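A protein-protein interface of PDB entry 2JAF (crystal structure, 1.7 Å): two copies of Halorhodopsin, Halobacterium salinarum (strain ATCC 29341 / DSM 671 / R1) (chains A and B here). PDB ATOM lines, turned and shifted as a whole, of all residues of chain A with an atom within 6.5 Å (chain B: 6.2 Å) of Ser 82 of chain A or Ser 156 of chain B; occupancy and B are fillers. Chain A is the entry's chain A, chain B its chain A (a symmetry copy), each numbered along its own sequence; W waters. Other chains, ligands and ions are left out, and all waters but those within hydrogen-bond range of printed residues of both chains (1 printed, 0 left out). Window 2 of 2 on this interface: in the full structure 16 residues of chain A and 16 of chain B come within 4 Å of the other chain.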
ATOM      1  N   ALA A  22      -1.534   8.089 -33.941  1.00  0.00           N
ATOM      2  CA  ALA A  22      -2.795   8.878 -33.823  1.00  0.00           C
ATOM      3  C   ALA A  22      -3.759   8.519 -34.949  1.00  0.00           C
ATOM      4  O   ALA A  22      -4.755   7.822 -34.736  1.00  0.00           O
ATOM      5  CB  ALA A  22      -2.477  10.371 -33.860  1.00  0.00           C
ATOM      6  N   ARG A  24      -5.566   6.823 -38.085  1.00  0.00           N
ATOM      7  CA  ARG A  24      -5.819   5.420 -38.354  1.00  0.00           C
ATOM      8  C   ARG A  24      -6.716   5.286 -39.579  1.00  0.00           C
ATOM      9  O   ARG A  24      -7.907   5.595 -39.523  1.00  0.00           O
ATOM     10  CB  ARG A  24      -6.483   4.750 -37.139  1.00  0.00           C
ATOM     11  CG  ARG A  24      -6.696   3.245 -37.299  1.00  0.00           C
ATOM     12  CD  ARG A  24      -7.500   2.621 -36.150  1.00  0.00           C
ATOM     13  NE  ARG A  24      -6.771   2.545 -34.882  1.00  0.00           N
ATOM     14  CZ  ARG A  24      -7.065   3.272 -33.807  1.00  0.00           C
ATOM     15  NH1 ARG A  24      -8.073   4.136 -33.845  1.00  0.00           N
ATOM     16  NH2 ARG A  24      -6.360   3.132 -32.688  1.00  0.00           N
ATOM     17  N   TYR A  77     -10.948  -0.675 -24.862  1.00  0.00           N
ATOM     18  CA  TYR A  77     -11.136  -0.362 -26.262  1.00  0.00           C
ATOM     19  C   TYR A  77     -11.227   1.140 -26.547  1.00  0.00           C
ATOM     20  O   TYR A  77     -10.796   1.591 -27.608  1.00  0.00           O
ATOM     21  CB  TYR A  77     -12.345  -1.131 -26.803  1.00  0.00           C
ATOM     22  CG  TYR A  77     -12.000  -2.588 -27.052  1.00  0.00           C
ATOM     23  CD1 TYR A  77     -11.260  -2.967 -28.176  1.00  0.00           C
ATOM     24  CD2 TYR A  77     -12.338  -3.573 -26.123  1.00  0.00           C
ATOM     25  CE1 TYR A  77     -10.858  -4.293 -28.368  1.00  0.00           C
ATOM     26  CE2 TYR A  77     -11.938  -4.903 -26.305  1.00  0.00           C
ATOM     27  CZ  TYR A  77     -11.200  -5.252 -27.424  1.00  0.00           C
ATOM     28  OH  TYR A  77     -10.784  -6.557 -27.587  1.00  0.00           O
ATOM     29  N   LEU A  78     -11.763   1.908 -25.607  1.00  0.00           N
ATOM     30  CA  LEU A  78     -11.837   3.360 -25.783  1.00  0.00           C
ATOM     31  C   LEU A  78     -10.412   3.918 -25.749  1.00  0.00           C
ATOM     32  O   LEU A  78     -10.074   4.840 -26.488  1.00  0.00           O
ATOM     33  CB  LEU A  78     -12.654   4.003 -24.658  1.00  0.00           C
ATOM     34  CG  LEU A  78     -14.127   3.612 -24.557  1.00  0.00           C
ATOM     35  CD1 LEU A  78     -14.744   4.279 -23.328  1.00  0.00           C
ATOM     36  CD2 LEU A  78     -14.859   4.030 -25.832  1.00  0.00           C
ATOM     37  N   GLY A  79      -9.585   3.358 -24.874  1.00  0.00           N
ATOM     38  CA  GLY A  79      -8.206   3.808 -24.778  1.00  0.00           C
ATOM     39  C   GLY A  79      -7.515   3.580 -26.108  1.00  0.00           C
ATOM     40  O   GLY A  79      -6.784   4.444 -26.604  1.00  0.00           O
ATOM     41  N   LEU A  80      -7.760   2.412 -26.699  1.00  0.00           N
ATOM     42  CA  LEU A  80      -7.163   2.077 -27.987  1.00  0.00           C
ATOM     43  C   LEU A  80      -7.719   2.938 -29.120  1.00  0.00           C
ATOM     44  O   LEU A  80      -6.968   3.533 -29.888  1.00  0.00           O
ATOM     45  CB  LEU A  80      -7.402   0.596 -28.308  1.00  0.00           C
ATOM     46  CG  LEU A  80      -6.819  -0.412 -27.311  1.00  0.00           C
ATOM     47  CD1 LEU A  80      -7.165  -1.835 -27.754  1.00  0.00           C
ATOM     48  CD2 LEU A  80      -5.311  -0.230 -27.217  1.00  0.00           C
ATOM     49  N   LEU A  81      -9.042   2.993 -29.225  1.00  0.00           N
ATOM     50  CA  LEU A  81      -9.684   3.778 -30.273  1.00  0.00           C
ATOM     51  C   LEU A  81      -9.226   5.230 -30.268  1.00  0.00           C
ATOM     52  O   LEU A  81      -8.925   5.803 -31.322  1.00  0.00           O
ATOM     53  CB  LEU A  81     -11.209   3.717 -30.112  1.00  0.00           C
ATOM     54  CG  LEU A  81     -11.908   2.506 -30.740  1.00  0.00           C
ATOM     55  CD1 LEU A  81     -13.385   2.500 -30.371  1.00  0.00           C
ATOM     56  CD2 LEU A  81     -11.734   2.559 -32.252  1.00  0.00           C
ATOM     57  N   SER A  82      -9.165   5.818 -29.078  1.00  0.00           N
ATOM     58  CA  SER A  82      -8.761   7.212 -28.929  1.00  0.00           C
ATOM     59  C   SER A  82      -7.277   7.447 -29.193  1.00  0.00           C
ATOM     60  O   SER A  82      -6.854   8.587 -29.395  1.00  0.00           O
ATOM     61  CB  SER A  82      -9.083   7.698 -27.521  1.00  0.00           C
ATOM     62  OG  SER A  82      -8.152   7.172 -26.593  1.00  0.00           O
ATOM     63  N   GLY A  83      -6.488   6.377 -29.180  1.00  0.00           N
ATOM     64  CA  GLY A  83      -5.058   6.521 -29.399  1.00  0.00           C
ATOM     65  C   GLY A  83      -4.305   6.789 -28.104  1.00  0.00           C
ATOM     66  O   GLY A  83      -3.077   6.812 -28.087  1.00  0.00           O
ATOM     67  N   LEU A  84      -5.035   6.982 -27.008  1.00  0.00           N
ATOM     68  CA  LEU A  84      -4.403   7.255 -25.719  1.00  0.00           C
ATOM     69  C   LEU A  84      -3.421   6.162 -25.314  1.00  0.00           C
ATOM     70  O   LEU A  84      -2.312   6.446 -24.862  1.00  0.00           O
ATOM     71  CB  LEU A  84      -5.467   7.402 -24.622  1.00  0.00           C
ATOM     72  CG  LEU A  84      -4.928   7.583 -23.193  1.00  0.00           C
ATOM     73  CD1 LEU A  84      -4.261   8.946 -23.072  1.00  0.00           C
ATOM     74  CD2 LEU A  84      -6.067   7.467 -22.177  1.00  0.00           C
ATOM     75  N   THR A  85      -3.825   4.907 -25.492  1.00  0.00           N
ATOM     76  CA  THR A  85      -2.985   3.783 -25.101  1.00  0.00           C
ATOM     77  C   THR A  85      -2.402   2.979 -26.266  1.00  0.00           C
ATOM     78  O   THR A  85      -2.278   1.754 -26.195  1.00  0.00           O
ATOM     79  CB  THR A  85      -3.764   2.841 -24.151  1.00  0.00           C
ATOM     80  OG1 THR A  85      -4.978   2.423 -24.782  1.00  0.00           O
ATOM     81  CG2 THR A  85      -4.106   3.561 -22.853  1.00  0.00           C
ATOM     82  N   VAL A  86      -2.044   3.683 -27.337  1.00  0.00           N
ATOM     83  CA  VAL A  86      -1.439   3.066 -28.512  1.00  0.00           C
ATOM     84  C   VAL A  86      -0.185   3.873 -28.802  1.00  0.00           C
ATOM     85  O   VAL A  86      -0.193   5.093 -28.671  1.00  0.00           O
ATOM     86  CB  VAL A  86      -2.360   3.135 -29.751  1.00  0.00           C
ATOM     87  CG1 VAL A  86      -1.685   2.449 -30.937  1.00  0.00           C
ATOM     88  CG2 VAL A  86      -3.687   2.466 -29.456  1.00  0.00           C
ATOM     89  N   PRO B  92      -9.120  19.206 -27.380  1.00  0.00           N
ATOM     90  CA  PRO B  92      -9.557  18.841 -28.734  1.00  0.00           C
ATOM     91  C   PRO B  92     -10.678  19.703 -29.296  1.00  0.00           C
ATOM     92  O   PRO B  92     -11.353  20.415 -28.557  1.00  0.00           O
ATOM     93  CB  PRO B  92     -10.001  17.393 -28.564  1.00  0.00           C
ATOM     94  CG  PRO B  92     -10.625  17.423 -27.204  1.00  0.00           C
ATOM     95  CD  PRO B  92      -9.611  18.224 -26.394  1.00  0.00           C
ATOM     96  N   ALA B  93     -10.869  19.623 -30.611  1.00  0.00           N
ATOM     97  CA  ALA B  93     -11.920  20.375 -31.290  1.00  0.00           C
ATOM     98  C   ALA B  93     -13.262  20.123 -30.606  1.00  0.00           C
ATOM     99  O   ALA B  93     -13.563  18.994 -30.201  1.00  0.00           O
ATOM    100  CB  ALA B  93     -11.996  19.955 -32.754  1.00  0.00           C
ATOM    101  N   MET B 153      -6.592  12.804 -19.649  1.00  0.00           N
ATOM    102  CA  MET B 153      -5.425  12.665 -20.526  1.00  0.00           C
ATOM    103  C   MET B 153      -5.721  12.498 -22.016  1.00  0.00           C
ATOM    104  O   MET B 153      -4.826  12.665 -22.847  1.00  0.00           O
ATOM    105  CB  MET B 153      -4.565  11.486 -20.066  1.00  0.00           C
ATOM    106  CG  MET B 153      -3.988  11.639 -18.668  1.00  0.00           C
ATOM    107  SD  MET B 153      -2.876  13.052 -18.496  1.00  0.00           S
ATOM    108  CE  MET B 153      -4.025  14.317 -17.838  1.00  0.00           C
ATOM    109  N   THR B 154      -6.964  12.162 -22.358  1.00  0.00           N
ATOM    110  CA  THR B 154      -7.338  11.955 -23.755  1.00  0.00           C
ATOM    111  C   THR B 154      -7.395  13.271 -24.535  1.00  0.00           C
ATOM    112  O   THR B 154      -8.066  14.212 -24.126  1.00  0.00           O
ATOM    113  CB  THR B 154      -8.688  11.225 -23.829  1.00  0.00           C
ATOM    114  OG1 THR B 154      -8.523   9.906 -23.292  1.00  0.00           O
ATOM    115  CG2 THR B 154      -9.188  11.133 -25.278  1.00  0.00           C
ATOM    116  N   THR B 155      -6.693  13.327 -25.664  1.00  0.00           N
ATOM    117  CA  THR B 155      -6.644  14.551 -26.456  1.00  0.00           C
ATOM    118  C   THR B 155      -7.076  14.432 -27.911  1.00  0.00           C
ATOM    119  O   THR B 155      -7.243  15.453 -28.587  1.00  0.00           O
ATOM    120  CB  THR B 155      -5.219  15.126 -26.476  1.00  0.00           C
ATOM    121  OG1 THR B 155      -4.334  14.163 -27.064  1.00  0.00           O
ATOM    122  CG2 THR B 155      -4.748  15.450 -25.066  1.00  0.00           C
ATOM    123  N   SER B 156      -7.267  13.211 -28.402  1.00  0.00           N
ATOM    124  CA  SER B 156      -7.618  13.041 -29.811  1.00  0.00           C
ATOM    125  C   SER B 156      -9.005  13.531 -30.203  1.00  0.00           C
ATOM    126  O   SER B 156      -9.178  14.116 -31.277  1.00  0.00           O
ATOM    127  CB  SER B 156      -7.436  11.576 -30.242  1.00  0.00           C
ATOM    128  OG  SER B 156      -8.367  10.719 -29.601  1.00  0.00           O
ATOM    129  N   ALA B 157      -9.994  13.304 -29.342  1.00  0.00           N
ATOM    130  CA  ALA B 157     -11.350  13.736 -29.632  1.00  0.00           C
ATOM    131  C   ALA B 157     -12.164  13.970 -28.365  1.00  0.00           C
ATOM    132  O   ALA B 157     -12.014  13.252 -27.380  1.00  0.00           O
ATOM    133  CB  ALA B 157     -12.051  12.698 -30.527  1.00  0.00           C
ATOM    134  N   LEU B 158     -13.026  14.980 -28.405  1.00  0.00           N
ATOM    135  CA  LEU B 158     -13.882  15.323 -27.278  1.00  0.00           C
ATOM    136  C   LEU B 158     -14.757  14.125 -26.899  1.00  0.00           C
ATOM    137  O   LEU B 158     -14.987  13.853 -25.720  1.00  0.00           O
ATOM    138  CB  LEU B 158     -14.763  16.531 -27.643  1.00  0.00           C
ATOM    139  CG  LEU B 158     -15.546  17.221 -26.521  1.00  0.00           C
ATOM    140  CD1 LEU B 158     -14.582  17.703 -25.434  1.00  0.00           C
ATOM    141  CD2 LEU B 158     -16.331  18.402 -27.092  1.00  0.00           C
ATOM    142  N   PHE B 160     -14.200  10.905 -26.871  1.00  0.00           N
ATOM    143  CA  PHE B 160     -13.554   9.942 -25.989  1.00  0.00           C
ATOM    144  C   PHE B 160     -13.343  10.461 -24.569  1.00  0.00           C
ATOM    145  O   PHE B 160     -13.390   9.682 -23.614  1.00  0.00           O
ATOM    146  CB  PHE B 160     -12.235   9.476 -26.605  1.00  0.00           C
ATOM    147  CG  PHE B 160     -12.416   8.745 -27.907  1.00  0.00           C
ATOM    148  CD1 PHE B 160     -13.148   7.564 -27.955  1.00  0.00           C
ATOM    149  CD2 PHE B 160     -11.866   9.243 -29.086  1.00  0.00           C
ATOM    150  CE1 PHE B 160     -13.335   6.884 -29.163  1.00  0.00           C
ATOM    151  CE2 PHE B 160     -12.045   8.571 -30.302  1.00  0.00           C
ATOM    152  CZ  PHE B 160     -12.778   7.395 -30.343  1.00  0.00           C
ATOM    153  N   PHE B 164     -15.088   8.344 -21.441  1.00  0.00           N
ATOM    154  CA  PHE B 164     -14.380   7.863 -20.253  1.00  0.00           C
ATOM    155  C   PHE B 164     -15.084   8.388 -18.997  1.00  0.00           C
ATOM    156  O   PHE B 164     -15.199   7.682 -17.989  1.00  0.00           O
ATOM    157  CB  PHE B 164     -12.919   8.331 -20.249  1.00  0.00           C
ATOM    158  CG  PHE B 164     -11.974   7.414 -20.989  1.00  0.00           C
ATOM    159  CD1 PHE B 164     -11.856   6.071 -20.630  1.00  0.00           C
ATOM    160  CD2 PHE B 164     -11.177   7.902 -22.027  1.00  0.00           C
ATOM    161  CE1 PHE B 164     -10.952   5.223 -21.291  1.00  0.00           C
ATOM    162  CE2 PHE B 164     -10.271   7.065 -22.696  1.00  0.00           C
ATOM    163  CZ  PHE B 164     -10.160   5.725 -22.327  1.00  0.00           C
HETATM  164  O   HOH W   1      -5.771  10.730 -27.075  1.00  0.00           O
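The side-chain hydroxyl (OG) of Ser 156 of chain B is in hydrogen-bond range of the backbone carbonyl oxygen (O) of Ser 82 of chain A (2.6 Å).
NH1 of Arg 24 of chain A is in hydrogen-bond range of O of Leu 81 of chain A (3.1 Å). The backbone carbonyl oxygen (O) of Leu 78 of chain A is in hydrogen-bond range of the side-chain hydroxyl (OG) of Ser 82 of chain A (3.0 Å). O of Gly 79 of chain A is in hydrogen-bond range of OG of Ser 82 of chain A (3.1 Å). The backbone carbonyl oxygen of Gly 79 of chain A lies within hydrogen-bond range of the backbone NH of Leu 84 of chain A (3.1 Å). The backbone carbonyl oxygen of Gly 79 of chain A is in hydrogen-bond range of the backbone NH of Thr 85 of chain A, at 3.2 Å. N of Leu 84 of chain A sits at hydrogen-bond distance from OG of Ser 82 of chain A, 3.2 Å away.
Phe 164 of chain B touches Leu 78 of chain A (CZ to CB, 3.8 Å). Phe 164 of chain B touches Gly 79 of chain A. CB of Leu 81 of chain A touches CE1 of Phe 160 of chain B, 3.9 Å away. Ser 82 of chain A touches Phe 160 of chain B. CD1 of Leu 84 of chain A touches O of Met 153 of chain B, 3.8 Å away. Leu 84 of chain A touches Thr 154 of chain B (CD2 to OG1, 3.6 Å).
Printed residues of chain B within 4 Å of Gly 79 of chain A: Phe 164. Of chain B, only Ser 156 and Phe 160 come within 4 Å of Ser 82 of chain A. Printed residues of chain A within 4 Å of Met 153 of chain B: Leu 84 (3.8 Å). Of the printed residues of chain A, Thr 154 of chain B touches Leu 84. Ser 156 of chain B touches just one residue of chain A: Ser 82 (2.6 Å). Printed residues of chain A within 4 Å of Phe 160 of chain B: Leu 81 and Ser 82. Of the printed residues of chain A, Phe 164 of chain B touches Leu 78 (3.8 Å) and Gly 79 (3.5 Å). The nearest residue of chain B that does not touch Ser 82 of chain A is Thr 154 of chain B (4.1 Å). The nearest residue of chain A that does not touch Ser 156 of chain B is Gly 83 of chain A (4.7 Å).
Of the 10 printed residues of chain B, 5 touch a printed residue of chain A. Printed residues of chain B that touch a printed residue of chain A: Met 153, Thr 154, Ser 156, Phe 160 and Phe 164. Hydrophobic or aromatic side chains of chain B within 4 Å of the printed part of chain A: Met 153, Phe 160 and Phe 164. Hydrophobic or aromatic side chains of chain A within 4 Å of the printed part of chain B: Leu 78, Leu 81 and Leu 84. Among the printed residues, 7 pairs touch across the chains. Among the printed residues, no Asp or Glu carboxylate lies within 4 Å of a Lys or Arg side-chain nitrogen of the other chain.
No position is printed for both chains. Of the 7 pairs that touch across the chains among the printed residues, none has its exchanged pair printed and touching as well.
Water W1 lies within hydrogen-bond range of the backbone NH of Thr 155 of chain B (3.1 Å), the backbone NH of Ser 156 of chain B (3.2 Å) and the backbone carbonyl oxygen of Ser 82 of chain A (3.3 Å).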
